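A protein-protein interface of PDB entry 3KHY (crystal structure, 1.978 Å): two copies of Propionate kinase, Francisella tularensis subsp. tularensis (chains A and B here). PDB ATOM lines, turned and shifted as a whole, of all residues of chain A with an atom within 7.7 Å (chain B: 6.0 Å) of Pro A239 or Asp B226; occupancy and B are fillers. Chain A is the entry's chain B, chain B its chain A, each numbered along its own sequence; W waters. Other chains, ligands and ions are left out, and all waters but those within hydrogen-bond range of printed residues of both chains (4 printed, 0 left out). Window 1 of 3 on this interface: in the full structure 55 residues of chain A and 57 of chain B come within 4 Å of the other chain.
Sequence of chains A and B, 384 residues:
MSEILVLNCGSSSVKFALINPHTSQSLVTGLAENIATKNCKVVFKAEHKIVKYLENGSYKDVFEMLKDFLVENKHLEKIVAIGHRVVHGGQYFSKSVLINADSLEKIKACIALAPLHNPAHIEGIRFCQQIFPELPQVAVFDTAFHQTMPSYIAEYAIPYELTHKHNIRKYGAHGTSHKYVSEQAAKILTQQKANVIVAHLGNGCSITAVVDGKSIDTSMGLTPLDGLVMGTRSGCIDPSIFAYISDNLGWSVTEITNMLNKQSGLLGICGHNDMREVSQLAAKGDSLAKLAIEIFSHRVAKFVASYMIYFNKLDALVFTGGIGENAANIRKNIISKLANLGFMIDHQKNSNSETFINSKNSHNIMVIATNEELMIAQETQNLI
The side-chain hydroxyl (OG) of Ser A240 lies within hydrogen-bond range of the side-chain hydroxyl (OG1) of Thr B223, 2.7 Å away. The backbone NH (N) of Thr B223 sits at hydrogen-bond distance from the side-chain carboxylate (OD2) of Asp A238. The backbone NH (N) of Leu B222 sits at hydrogen-bond distance from the side-chain carboxylate (OD2) of Asp A238 (2.8 Å).
The backbone carbonyl oxygen (O) of Leu B225 sits close to the backbone NH (N) of Gly B235 (3.3 Å). O of Leu B260 is in hydrogen-bond range of N of Ser B234 (3.0 Å). OH of Tyr B156 sits at hydrogen-bond distance from N of Leu B222. The backbone NH of Leu B225 sits close to the side-chain hydroxyl of Thr B223 (3.1 Å). OD1 of Asp A238 is in hydrogen-bond range of OG of Ser A240, at 2.7 Å.
Ile A237 touches Tyr B156. Ile A237 touches Pro B239 (CG2 to CG, 3.96 Å). Tyr B156 touches Asp A238 (OH to CB, 3.4 Å). Gly B221 touches Asp A238 (C to OD2, 3.5 Å). CD of Pro A239 touches OD1 of Asp B226, 3.8 Å away. CD1 of Leu B260 touches CB of Pro A239, at 3.96 Å. CB of Leu B225 touches OG of Ser A240, at 3.5 Å. CB of Ala A243 touches OG1 of Thr B257, 3.7 Å away. Tyr A244 touches Leu B222 (CB to CD2, 3.8 Å). Pro B239 touches Leu A260 (CB to CD1, 3.8 Å).
Of chain B, only Leu B225 (3.6 Å), Asp B226 (3.8 Å), Ile B237 (3.9 Å), Phe B242 (3.5 Å) and Leu B260 (3.96 Å) come within 4 Å of Pro A239. Of the printed residues of chain A, Asp B226 touches Asp A238 (3.3 Å) and Pro A239 (3.8 Å). Printed residues of chain B within 4 Å of Ala A243: Thr B257 (3.7 Å). Printed residues of chain A within 4 Å of Ile B237: Pro A239 (3.9 Å). Of the printed residues of chain B, Ser A240 touches Thr B223 and Leu B225. Printed residues of chain A within 4 Å of Pro B239: Ile A237 (3.96 Å), Phe A242 (3.6 Å) and Leu A260 (3.8 Å). Lys B170 touches none of the printed residues of chain A. The nearest residue of chain B that does not touch Pro A239 is Gly B235 (4.4 Å). The nearest residue of chain A that does not touch Asp B226 is Ile A237 (4.2 Å). The nearest printed residue of chain A that does not touch Thr B257 is Phe A242 (5.1 Å).
Of the 11 printed residues of chain A, 8 touch a printed residue of chain B. Hydrophobic or aromatic side chains of chain A within 4 Å of the printed part of chain B: Ile A237, Pro A239, Phe A242, Ala A243, Tyr A244 and Leu A260. Of the 23 printed residues of chain B, 11 touch a printed residue of chain A. Printed residues of chain B that touch a printed residue of chain A: Tyr B156, Gly B221, Leu B222, Thr B223, Leu B225, Asp B226, Ile B237, Pro B239, Phe B242, Thr B257 and Leu B260. Among the printed residues, no Asp or Glu carboxylate lies within 4 Å of a Lys or Arg side-chain nitrogen of the other chain.
Ile A237 touches Pro B239, and with the chains exchanged Pro A239 touches Ile B237. Pro A239 touches Phe B242, and with the chains exchanged Phe A242 touches Pro B239. Pro A239 touches Leu B260, and with the chains exchanged Leu A260 touches Pro B239. Phe B242 touches its own counterpart, Phe A242. 6 positions are printed for both chains. Of the 19 pairs that touch across the chains among the printed residues, 7 have their exchanged pair printed and touching as well.
Water W2 lies within hydrogen-bond range of the side-chain carboxylate (OD1) of Asp B226, the backbone carbonyl oxygen (O) of Ile A237 and the backbone NH (N) of Ile B237. Water W1 lies within hydrogen-bond range of O of Pro A239, OG1 of Thr B257, N of Ala A243 and O of Ser A240. Water W4 lies within hydrogen-bond range of O of Ile A237 and O of Ile B237. Water W3 lies within hydrogen-bond range of O of Ile B237 (3.0 Å) and N of Ile A237 (3.1 Å).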
ATOM      1  N   CYS A 236      -7.012  13.806  -7.816  1.00  0.00           N
ATOM      2  CA  CYS A 236      -6.975  14.615  -9.046  1.00  0.00           C
ATOM      3  C   CYS A 236      -8.071  15.664  -9.152  1.00  0.00           C
ATOM      4  O   CYS A 236      -9.248  15.364  -8.944  1.00  0.00           O
ATOM      5  CB  CYS A 236      -7.082  13.718 -10.271  1.00  0.00           C
ATOM      6  SG  CYS A 236      -5.660  12.654 -10.437  1.00  0.00           S
ATOM      7  N   ILE A 237      -7.672  16.879  -9.518  1.00  0.00           N
ATOM      8  CA  ILE A 237      -8.615  17.968  -9.771  1.00  0.00           C
ATOM      9  C   ILE A 237      -7.976  19.050 -10.644  1.00  0.00           C
ATOM     10  O   ILE A 237      -6.750  19.228 -10.640  1.00  0.00           O
ATOM     11  CB  ILE A 237      -9.149  18.562  -8.453  1.00  0.00           C
ATOM     12  CG1 ILE A 237     -10.382  19.432  -8.701  1.00  0.00           C
ATOM     13  CG2 ILE A 237      -8.055  19.332  -7.707  1.00  0.00           C
ATOM     14  CD1 ILE A 237     -11.223  19.652  -7.435  1.00  0.00           C
ATOM     15  N   ASP A 238      -8.808  19.739 -11.424  1.00  0.00           N
ATOM     16  CA  ASP A 238      -8.356  20.810 -12.323  1.00  0.00           C
ATOM     17  C   ASP A 238      -7.768  21.936 -11.471  1.00  0.00           C
ATOM     18  O   ASP A 238      -8.446  22.443 -10.582  1.00  0.00           O
ATOM     19  CB  ASP A 238      -9.562  21.314 -13.142  1.00  0.00           C
ATOM     20  CG  ASP A 238      -9.201  22.407 -14.155  1.00  0.00           C
ATOM     21  OD1 ASP A 238      -8.091  22.968 -14.102  1.00  0.00           O
ATOM     22  OD2 ASP A 238     -10.057  22.724 -15.013  1.00  0.00           O
ATOM     23  N   PRO A 239      -6.500  22.314 -11.721  1.00  0.00           N
ATOM     24  CA  PRO A 239      -5.864  23.416 -10.983  1.00  0.00           C
ATOM     25  C   PRO A 239      -6.633  24.726 -11.146  1.00  0.00           C
ATOM     26  O   PRO A 239      -6.448  25.624 -10.337  1.00  0.00           O
ATOM     27  CB  PRO A 239      -4.489  23.546 -11.655  1.00  0.00           C
ATOM     28  CG  PRO A 239      -4.638  22.862 -12.986  1.00  0.00           C
ATOM     29  CD  PRO A 239      -5.571  21.712 -12.690  1.00  0.00           C
ATOM     30  N   SER A 240      -7.473  24.825 -12.175  1.00  0.00           N
ATOM     31  CA  SER A 240      -8.296  26.019 -12.380  1.00  0.00           C
ATOM     32  C   SER A 240      -9.202  26.331 -11.190  1.00  0.00           C
ATOM     33  O   SER A 240      -9.687  27.459 -11.051  1.00  0.00           O
ATOM     34  CB  SER A 240      -9.168  25.876 -13.639  1.00  0.00           C
ATOM     35  OG  SER A 240      -8.402  25.517 -14.766  1.00  0.00           O
ATOM     36  N   ILE A 241      -9.455  25.345 -10.335  1.00  0.00           N
ATOM     37  CA  ILE A 241     -10.389  25.567  -9.227  1.00  0.00           C
ATOM     38  C   ILE A 241      -9.900  26.624  -8.245  1.00  0.00           C
ATOM     39  O   ILE A 241     -10.710  27.290  -7.578  1.00  0.00           O
ATOM     40  CB  ILE A 241     -10.760  24.267  -8.472  1.00  0.00           C
ATOM     41  CG1 ILE A 241      -9.521  23.620  -7.848  1.00  0.00           C
ATOM     42  CG2 ILE A 241     -11.496  23.291  -9.408  1.00  0.00           C
ATOM     43  CD1 ILE A 241      -9.520  23.655  -6.333  1.00  0.00           C
ATOM     44  N   PHE A 242      -8.583  26.805  -8.165  1.00  0.00           N
ATOM     45  CA  PHE A 242      -8.044  27.793  -7.236  1.00  0.00           C
ATOM     46  C   PHE A 242      -8.487  29.202  -7.609  1.00  0.00           C
ATOM     47  O   PHE A 242      -9.029  29.922  -6.774  1.00  0.00           O
ATOM     48  CB  PHE A 242      -6.523  27.692  -7.110  1.00  0.00           C
ATOM     49  CG  PHE A 242      -6.075  26.590  -6.198  1.00  0.00           C
ATOM     50  CD1 PHE A 242      -5.751  26.851  -4.867  1.00  0.00           C
ATOM     51  CD2 PHE A 242      -6.019  25.287  -6.651  1.00  0.00           C
ATOM     52  CE1 PHE A 242      -5.354  25.832  -4.023  1.00  0.00           C
ATOM     53  CE2 PHE A 242      -5.625  24.258  -5.801  1.00  0.00           C
ATOM     54  CZ  PHE A 242      -5.287  24.532  -4.499  1.00  0.00           C
ATOM     55  N   ALA A 243      -8.260  29.591  -8.860  1.00  0.00           N
ATOM     56  CA  ALA A 243      -8.659  30.919  -9.322  1.00  0.00           C
ATOM     57  C   ALA A 243     -10.177  31.066  -9.253  1.00  0.00           C
ATOM     58  O   ALA A 243     -10.709  32.123  -8.896  1.00  0.00           O
ATOM     59  CB  ALA A 243      -8.166  31.158 -10.747  1.00  0.00           C
ATOM     60  N   TYR A 244     -10.877  30.003  -9.608  1.00  0.00           N
ATOM     61  CA  TYR A 244     -12.332  30.066  -9.626  1.00  0.00           C
ATOM     62  C   TYR A 244     -12.888  30.314  -8.216  1.00  0.00           C
ATOM     63  O   TYR A 244     -13.719  31.204  -8.001  1.00  0.00           O
ATOM     64  CB  TYR A 244     -12.922  28.797 -10.239  1.00  0.00           C
ATOM     65  CG  TYR A 244     -14.431  28.812 -10.280  1.00  0.00           C
ATOM     66  CD1 TYR A 244     -15.175  28.343  -9.212  1.00  0.00           C
ATOM     67  CD2 TYR A 244     -15.108  29.319 -11.384  1.00  0.00           C
ATOM     68  CE1 TYR A 244     -16.562  28.365  -9.243  1.00  0.00           C
ATOM     69  CE2 TYR A 244     -16.488  29.346 -11.426  1.00  0.00           C
ATOM     70  CZ  TYR A 244     -17.212  28.868 -10.355  1.00  0.00           C
ATOM     71  OH  TYR A 244     -18.586  28.894 -10.398  1.00  0.00           O
ATOM     72  N   ILE A 256      -8.355  26.869   0.463  1.00  0.00           N
ATOM     73  CA  ILE A 256      -8.713  25.944  -0.608  1.00  0.00           C
ATOM     74  C   ILE A 256      -7.959  24.626  -0.439  1.00  0.00           C
ATOM     75  O   ILE A 256      -8.532  23.549  -0.565  1.00  0.00           O
ATOM     76  CB  ILE A 256      -8.432  26.531  -1.992  1.00  0.00           C
ATOM     77  CG1 ILE A 256      -9.258  27.809  -2.193  1.00  0.00           C
ATOM     78  CG2 ILE A 256      -8.763  25.483  -3.092  1.00  0.00           C
ATOM     79  CD1 ILE A 256      -8.725  28.688  -3.339  1.00  0.00           C
ATOM     80  N   LEU A 260      -9.351  20.684   0.197  1.00  0.00           N
ATOM     81  CA  LEU A 260      -9.013  19.550  -0.661  1.00  0.00           C
ATOM     82  C   LEU A 260      -8.451  18.386   0.152  1.00  0.00           C
ATOM     83  O   LEU A 260      -8.657  17.221  -0.198  1.00  0.00           O
ATOM     84  CB  LEU A 260      -8.015  19.967  -1.761  1.00  0.00           C
ATOM     85  CG  LEU A 260      -8.547  20.933  -2.827  1.00  0.00           C
ATOM     86  CD1 LEU A 260      -7.415  21.386  -3.781  1.00  0.00           C
ATOM     87  CD2 LEU A 260      -9.707  20.330  -3.617  1.00  0.00           C
ATOM     88  N   TYR B 156     -16.010  16.034  -9.415  1.00  0.00           N
ATOM     89  CA  TYR B 156     -14.810  15.836  -8.606  1.00  0.00           C
ATOM     90  C   TYR B 156     -15.195  15.330  -7.212  1.00  0.00           C
ATOM     91  O   TYR B 156     -16.359  15.397  -6.826  1.00  0.00           O
ATOM     92  CB  TYR B 156     -14.035  17.144  -8.492  1.00  0.00           C
ATOM     93  CG  TYR B 156     -13.538  17.667  -9.828  1.00  0.00           C
ATOM     94  CD1 TYR B 156     -12.698  16.898 -10.628  1.00  0.00           C
ATOM     95  CD2 TYR B 156     -13.904  18.933 -10.281  1.00  0.00           C
ATOM     96  CE1 TYR B 156     -12.233  17.382 -11.847  1.00  0.00           C
ATOM     97  CE2 TYR B 156     -13.441  19.423 -11.484  1.00  0.00           C
ATOM     98  CZ  TYR B 156     -12.615  18.645 -12.268  1.00  0.00           C
ATOM     99  OH  TYR B 156     -12.165  19.136 -13.479  1.00  0.00           O
ATOM    100  N   LYS B 170     -16.036  18.763 -13.935  1.00  0.00           N
ATOM    101  CA  LYS B 170     -15.421  18.693 -15.243  1.00  0.00           C
ATOM    102  C   LYS B 170     -16.447  19.040 -16.324  1.00  0.00           C
ATOM    103  O   LYS B 170     -17.532  18.451 -16.356  1.00  0.00           O
ATOM    104  CB  LYS B 170     -14.883  17.283 -15.482  1.00  0.00           C
ATOM    105  CG  LYS B 170     -14.341  17.074 -16.909  1.00  0.00           C
ATOM    106  CD  LYS B 170     -13.786  15.668 -17.061  1.00  0.00           C
ATOM    107  CE  LYS B 170     -12.364  15.632 -16.516  1.00  0.00           C
ATOM    108  NZ  LYS B 170     -11.662  14.394 -16.855  1.00  0.00           N
ATOM    109  N   CYS B 205      -4.741  21.063 -26.351  1.00  0.00           N
ATOM    110  CA  CYS B 205      -4.798  19.617 -26.593  1.00  0.00           C
ATOM    111  C   CYS B 205      -5.783  18.975 -25.636  1.00  0.00           C
ATOM    112  O   CYS B 205      -5.744  19.232 -24.434  1.00  0.00           O
ATOM    113  CB  CYS B 205      -3.415  18.964 -26.383  1.00  0.00           C
ATOM    114  SG  CYS B 205      -2.128  19.526 -27.529  1.00  0.00           S
ATOM    115  N   SER B 219     -10.522  15.020 -21.270  1.00  0.00           N
ATOM    116  CA  SER B 219      -9.335  15.356 -20.475  1.00  0.00           C
ATOM    117  C   SER B 219      -9.296  16.773 -19.879  1.00  0.00           C
ATOM    118  O   SER B 219      -8.682  16.984 -18.829  1.00  0.00           O
ATOM    119  CB  SER B 219      -8.060  15.062 -21.268  1.00  0.00           C
ATOM    120  OG  SER B 219      -7.935  15.940 -22.368  1.00  0.00           O
ATOM    121  N   MET B 220      -9.931  17.748 -20.533  1.00  0.00           N
ATOM    122  CA  MET B 220      -9.992  19.099 -19.946  1.00  0.00           C
ATOM    123  C   MET B 220     -10.961  19.122 -18.763  1.00  0.00           C
ATOM    124  O   MET B 220     -11.701  18.176 -18.567  1.00  0.00           O
ATOM    125  CB  MET B 220     -10.347  20.155 -20.993  1.00  0.00           C
ATOM    126  CG  MET B 220      -9.163  20.489 -21.901  1.00  0.00           C
ATOM    127  SD  MET B 220      -9.705  21.466 -23.489  1.00  0.00           S
ATOM    128  CE  MET B 220      -7.936  22.085 -24.075  1.00  0.00           C
ATOM    129  N   GLY B 221     -10.952  20.175 -17.955  1.00  0.00           N
ATOM    130  CA  GLY B 221     -11.687  20.103 -16.700  1.00  0.00           C
ATOM    131  C   GLY B 221     -12.768  21.151 -16.593  1.00  0.00           C
ATOM    132  O   GLY B 221     -13.625  21.272 -17.475  1.00  0.00           O
ATOM    133  N   LEU B 222     -12.725  21.902 -15.504  1.00  0.00           N
ATOM    134  CA  LEU B 222     -13.572  23.085 -15.348  1.00  0.00           C
ATOM    135  C   LEU B 222     -13.315  24.041 -16.500  1.00  0.00           C
ATOM    136  O   LEU B 222     -14.250  24.579 -17.100  1.00  0.00           O
ATOM    137  CB  LEU B 222     -13.248  23.778 -14.020  1.00  0.00           C
ATOM    138  CG  LEU B 222     -14.050  25.015 -13.595  1.00  0.00           C
ATOM    139  CD1 LEU B 222     -15.453  24.607 -13.191  1.00  0.00           C
ATOM    140  CD2 LEU B 222     -13.345  25.684 -12.423  1.00  0.00           C
ATOM    141  N   THR B 223     -12.035  24.239 -16.812  1.00  0.00           N
ATOM    142  CA  THR B 223     -11.617  25.085 -17.929  1.00  0.00           C
ATOM    143  C   THR B 223     -10.693  24.295 -18.857  1.00  0.00           C
ATOM    144  O   THR B 223     -10.352  23.153 -18.556  1.00  0.00           O
ATOM    145  CB  THR B 223     -10.857  26.329 -17.439  1.00  0.00           C
ATOM    146  OG1 THR B 223      -9.494  25.975 -17.172  1.00  0.00           O
ATOM    147  CG2 THR B 223     -11.508  26.924 -16.188  1.00  0.00           C
ATOM    148  N   PRO B 224     -10.266  24.906 -19.980  1.00  0.00           N
ATOM    149  CA  PRO B 224      -9.335  24.236 -20.903  1.00  0.00           C
ATOM    150  C   PRO B 224      -7.867  24.156 -20.427  1.00  0.00           C
ATOM    151  O   PRO B 224      -6.996  23.819 -21.233  1.00  0.00           O
ATOM    152  CB  PRO B 224      -9.425  25.095 -22.186  1.00  0.00           C
ATOM    153  CG  PRO B 224     -10.733  25.867 -22.046  1.00  0.00           C
ATOM    154  CD  PRO B 224     -10.839  26.130 -20.570  1.00  0.00           C
ATOM    155  N   LEU B 225      -7.595  24.449 -19.159  1.00  0.00           N
ATOM    156  CA  LEU B 225      -6.238  24.296 -18.610  1.00  0.00           C
ATOM    157  C   LEU B 225      -5.830  22.835 -18.329  1.00  0.00           C
ATOM    158  O   LEU B 225      -4.654  22.484 -18.430  1.00  0.00           O
ATOM    159  CB  LEU B 225      -6.105  25.097 -17.315  1.00  0.00           C
ATOM    160  CG  LEU B 225      -4.808  24.903 -16.525  1.00  0.00           C
ATOM    161  CD1 LEU B 225      -3.597  25.342 -17.350  1.00  0.00           C
ATOM    162  CD2 LEU B 225      -4.879  25.674 -15.224  1.00  0.00           C
ATOM    163  N   ASP B 226      -6.792  21.990 -17.971  1.00  0.00           N
ATOM    164  CA  ASP B 226      -6.477  20.660 -17.428  1.00  0.00           C
ATOM    165  C   ASP B 226      -6.207  19.592 -18.492  1.00  0.00           C
ATOM    166  O   ASP B 226      -6.605  19.730 -19.662  1.00  0.00           O
ATOM    167  CB  ASP B 226      -7.624  20.174 -16.547  1.00  0.00           C
ATOM    168  CG  ASP B 226      -7.173  19.176 -15.475  1.00  0.00           C
ATOM    169  OD1 ASP B 226      -5.945  18.961 -15.299  1.00  0.00           O
ATOM    170  OD2 ASP B 226      -8.059  18.613 -14.804  1.00  0.00           O
ATOM    171  N   GLY B 227      -5.554  18.512 -18.069  1.00  0.00           N
ATOM    172  CA  GLY B 227      -5.397  17.334 -18.902  1.00  0.00           C
ATOM    173  C   GLY B 227      -4.045  17.177 -19.576  1.00  0.00           C
ATOM    174  O   GLY B 227      -3.002  17.064 -18.908  1.00  0.00           O
ATOM    175  N   LEU B 228      -4.071  17.157 -20.904  1.00  0.00           N
ATOM    176  CA  LEU B 228      -2.871  16.943 -21.724  1.00  0.00           C
ATOM    177  C   LEU B 228      -1.868  18.093 -21.642  1.00  0.00           C
ATOM    178  O   LEU B 228      -2.243  19.239 -21.348  1.00  0.00           O
ATOM    179  CB  LEU B 228      -3.276  16.727 -23.196  1.00  0.00           C
ATOM    180  CG  LEU B 228      -4.130  15.494 -23.494  1.00  0.00           C
ATOM    181  CD1 LEU B 228      -4.378  15.341 -25.022  1.00  0.00           C
ATOM    182  CD2 LEU B 228      -3.470  14.231 -22.918  1.00  0.00           C
ATOM    183  N   MET B 230       0.220  20.971 -23.264  1.00  0.00           N
ATOM    184  CA  MET B 230      -0.104  21.838 -24.398  1.00  0.00           C
ATOM    185  C   MET B 230       1.038  22.822 -24.701  1.00  0.00           C
ATOM    186  O   MET B 230       2.104  22.738 -24.102  1.00  0.00           O
ATOM    187  CB  MET B 230      -1.424  22.577 -24.145  1.00  0.00           C
ATOM    188  CG  MET B 230      -2.449  21.730 -23.401  1.00  0.00           C
ATOM    189  SD  MET B 230      -4.239  22.563 -23.270  1.00  0.00           S
ATOM    190  CE  MET B 230      -4.978  21.392 -21.881  1.00  0.00           C
ATOM    191  N   SER B 234      -0.008  23.703 -18.620  1.00  0.00           N
ATOM    192  CA  SER B 234       0.551  22.564 -17.903  1.00  0.00           C
ATOM    193  C   SER B 234      -0.230  21.261 -18.059  1.00  0.00           C
ATOM    194  O   SER B 234       0.350  20.173 -18.005  1.00  0.00           O
ATOM    195  CB  SER B 234       0.606  22.896 -16.412  1.00  0.00           C
ATOM    196  OG  SER B 234      -0.709  23.030 -15.881  1.00  0.00           O
ATOM    197  N   GLY B 235      -1.543  21.367 -18.232  1.00  0.00           N
ATOM    198  CA  GLY B 235      -2.408  20.206 -18.101  1.00  0.00           C
ATOM    199  C   GLY B 235      -2.367  19.706 -16.663  1.00  0.00           C
ATOM    200  O   GLY B 235      -2.113  20.488 -15.743  1.00  0.00           O
ATOM    201  N   CYS B 236      -2.617  18.410 -16.476  1.00  0.00           N
ATOM    202  CA  CYS B 236      -2.651  17.781 -15.152  1.00  0.00           C
ATOM    203  C   CYS B 236      -1.493  18.175 -14.251  1.00  0.00           C
ATOM    204  O   CYS B 236      -0.335  18.117 -14.661  1.00  0.00           O
ATOM    205  CB  CYS B 236      -2.613  16.260 -15.300  1.00  0.00           C
ATOM    206  SG  CYS B 236      -4.124  15.566 -15.977  1.00  0.00           S
ATOM    207  N   ILE B 237      -1.809  18.537 -13.013  1.00  0.00           N
ATOM    208  CA  ILE B 237      -0.775  18.813 -12.018  1.00  0.00           C
ATOM    209  C   ILE B 237      -1.364  18.698 -10.602  1.00  0.00           C
ATOM    210  O   ILE B 237      -2.568  18.866 -10.406  1.00  0.00           O
ATOM    211  CB  ILE B 237      -0.143  20.203 -12.254  1.00  0.00           C
ATOM    212  CG1 ILE B 237       1.094  20.415 -11.382  1.00  0.00           C
ATOM    213  CG2 ILE B 237      -1.164  21.323 -12.006  1.00  0.00           C
ATOM    214  CD1 ILE B 237       1.951  21.574 -11.887  1.00  0.00           C
ATOM    215  N   PRO B 239      -2.675  19.662  -7.251  1.00  0.00           N
ATOM    216  CA  PRO B 239      -3.209  20.939  -6.759  1.00  0.00           C
ATOM    217  C   PRO B 239      -2.338  21.513  -5.643  1.00  0.00           C
ATOM    218  O   PRO B 239      -2.370  22.717  -5.396  1.00  0.00           O
ATOM    219  CB  PRO B 239      -4.587  20.554  -6.204  1.00  0.00           C
ATOM    220  CG  PRO B 239      -4.506  19.040  -5.977  1.00  0.00           C
ATOM    221  CD  PRO B 239      -3.642  18.563  -7.095  1.00  0.00           C
ATOM    222  N   ILE B 241       0.529  22.305  -5.656  1.00  0.00           N
ATOM    223  CA  ILE B 241       1.544  23.244  -6.114  1.00  0.00           C
ATOM    224  C   ILE B 241       1.183  24.687  -5.751  1.00  0.00           C
ATOM    225  O   ILE B 241       2.065  25.535  -5.654  1.00  0.00           O
ATOM    226  CB  ILE B 241       1.880  23.119  -7.630  1.00  0.00           C
ATOM    227  CG1 ILE B 241       0.647  23.332  -8.504  1.00  0.00           C
ATOM    228  CG2 ILE B 241       2.505  21.762  -7.936  1.00  0.00           C
ATOM    229  CD1 ILE B 241       0.430  24.769  -8.904  1.00  0.00           C
ATOM    230  N   PHE B 242      -0.102  24.962  -5.537  1.00  0.00           N
ATOM    231  CA  PHE B 242      -0.513  26.324  -5.226  1.00  0.00           C
ATOM    232  C   PHE B 242       0.017  26.743  -3.857  1.00  0.00           C
ATOM    233  O   PHE B 242       0.643  27.790  -3.728  1.00  0.00           O
ATOM    234  CB  PHE B 242      -2.027  26.493  -5.324  1.00  0.00           C
ATOM    235  CG  PHE B 242      -2.519  26.675  -6.742  1.00  0.00           C
ATOM    236  CD1 PHE B 242      -2.816  27.933  -7.235  1.00  0.00           C
ATOM    237  CD2 PHE B 242      -2.650  25.589  -7.584  1.00  0.00           C
ATOM    238  CE1 PHE B 242      -3.261  28.099  -8.559  1.00  0.00           C
ATOM    239  CE2 PHE B 242      -3.094  25.750  -8.906  1.00  0.00           C
ATOM    240  CZ  PHE B 242      -3.398  27.006  -9.382  1.00  0.00           C
ATOM    241  N   THR B 257      -1.720  30.850 -11.456  1.00  0.00           N
ATOM    242  CA  THR B 257      -2.612  30.382 -12.508  1.00  0.00           C
ATOM    243  C   THR B 257      -2.131  30.870 -13.872  1.00  0.00           C
ATOM    244  O   THR B 257      -2.189  30.135 -14.868  1.00  0.00           O
ATOM    245  CB  THR B 257      -4.064  30.855 -12.273  1.00  0.00           C
ATOM    246  OG1 THR B 257      -4.540  30.357 -11.016  1.00  0.00           O
ATOM    247  CG2 THR B 257      -4.986  30.354 -13.390  1.00  0.00           C
ATOM    248  N   LEU B 260       0.668  28.665 -15.014  1.00  0.00           N
ATOM    249  CA  LEU B 260       0.224  27.363 -15.517  1.00  0.00           C
ATOM    250  C   LEU B 260      -0.426  27.463 -16.890  1.00  0.00           C
ATOM    251  O   LEU B 260      -0.406  26.509 -17.659  1.00  0.00           O
ATOM    252  CB  LEU B 260      -0.755  26.714 -14.539  1.00  0.00           C
ATOM    253  CG  LEU B 260      -0.204  26.242 -13.192  1.00  0.00           C
ATOM    254  CD1 LEU B 260      -1.352  25.881 -12.267  1.00  0.00           C
ATOM    255  CD2 LEU B 260       0.723  25.022 -13.385  1.00  0.00           C
HETATM  256  O   HOH W   1      -6.456  28.331 -10.723  1.00  0.00           O
HETATM  257  O   HOH W   2      -4.935  18.262 -12.855  1.00  0.00           O
HETATM  258  O   HOH W   3      -4.613  16.731  -9.983  1.00  0.00           O
HETATM  259  O   HOH W   4      -4.614  20.757  -9.631  1.00  0.00           O
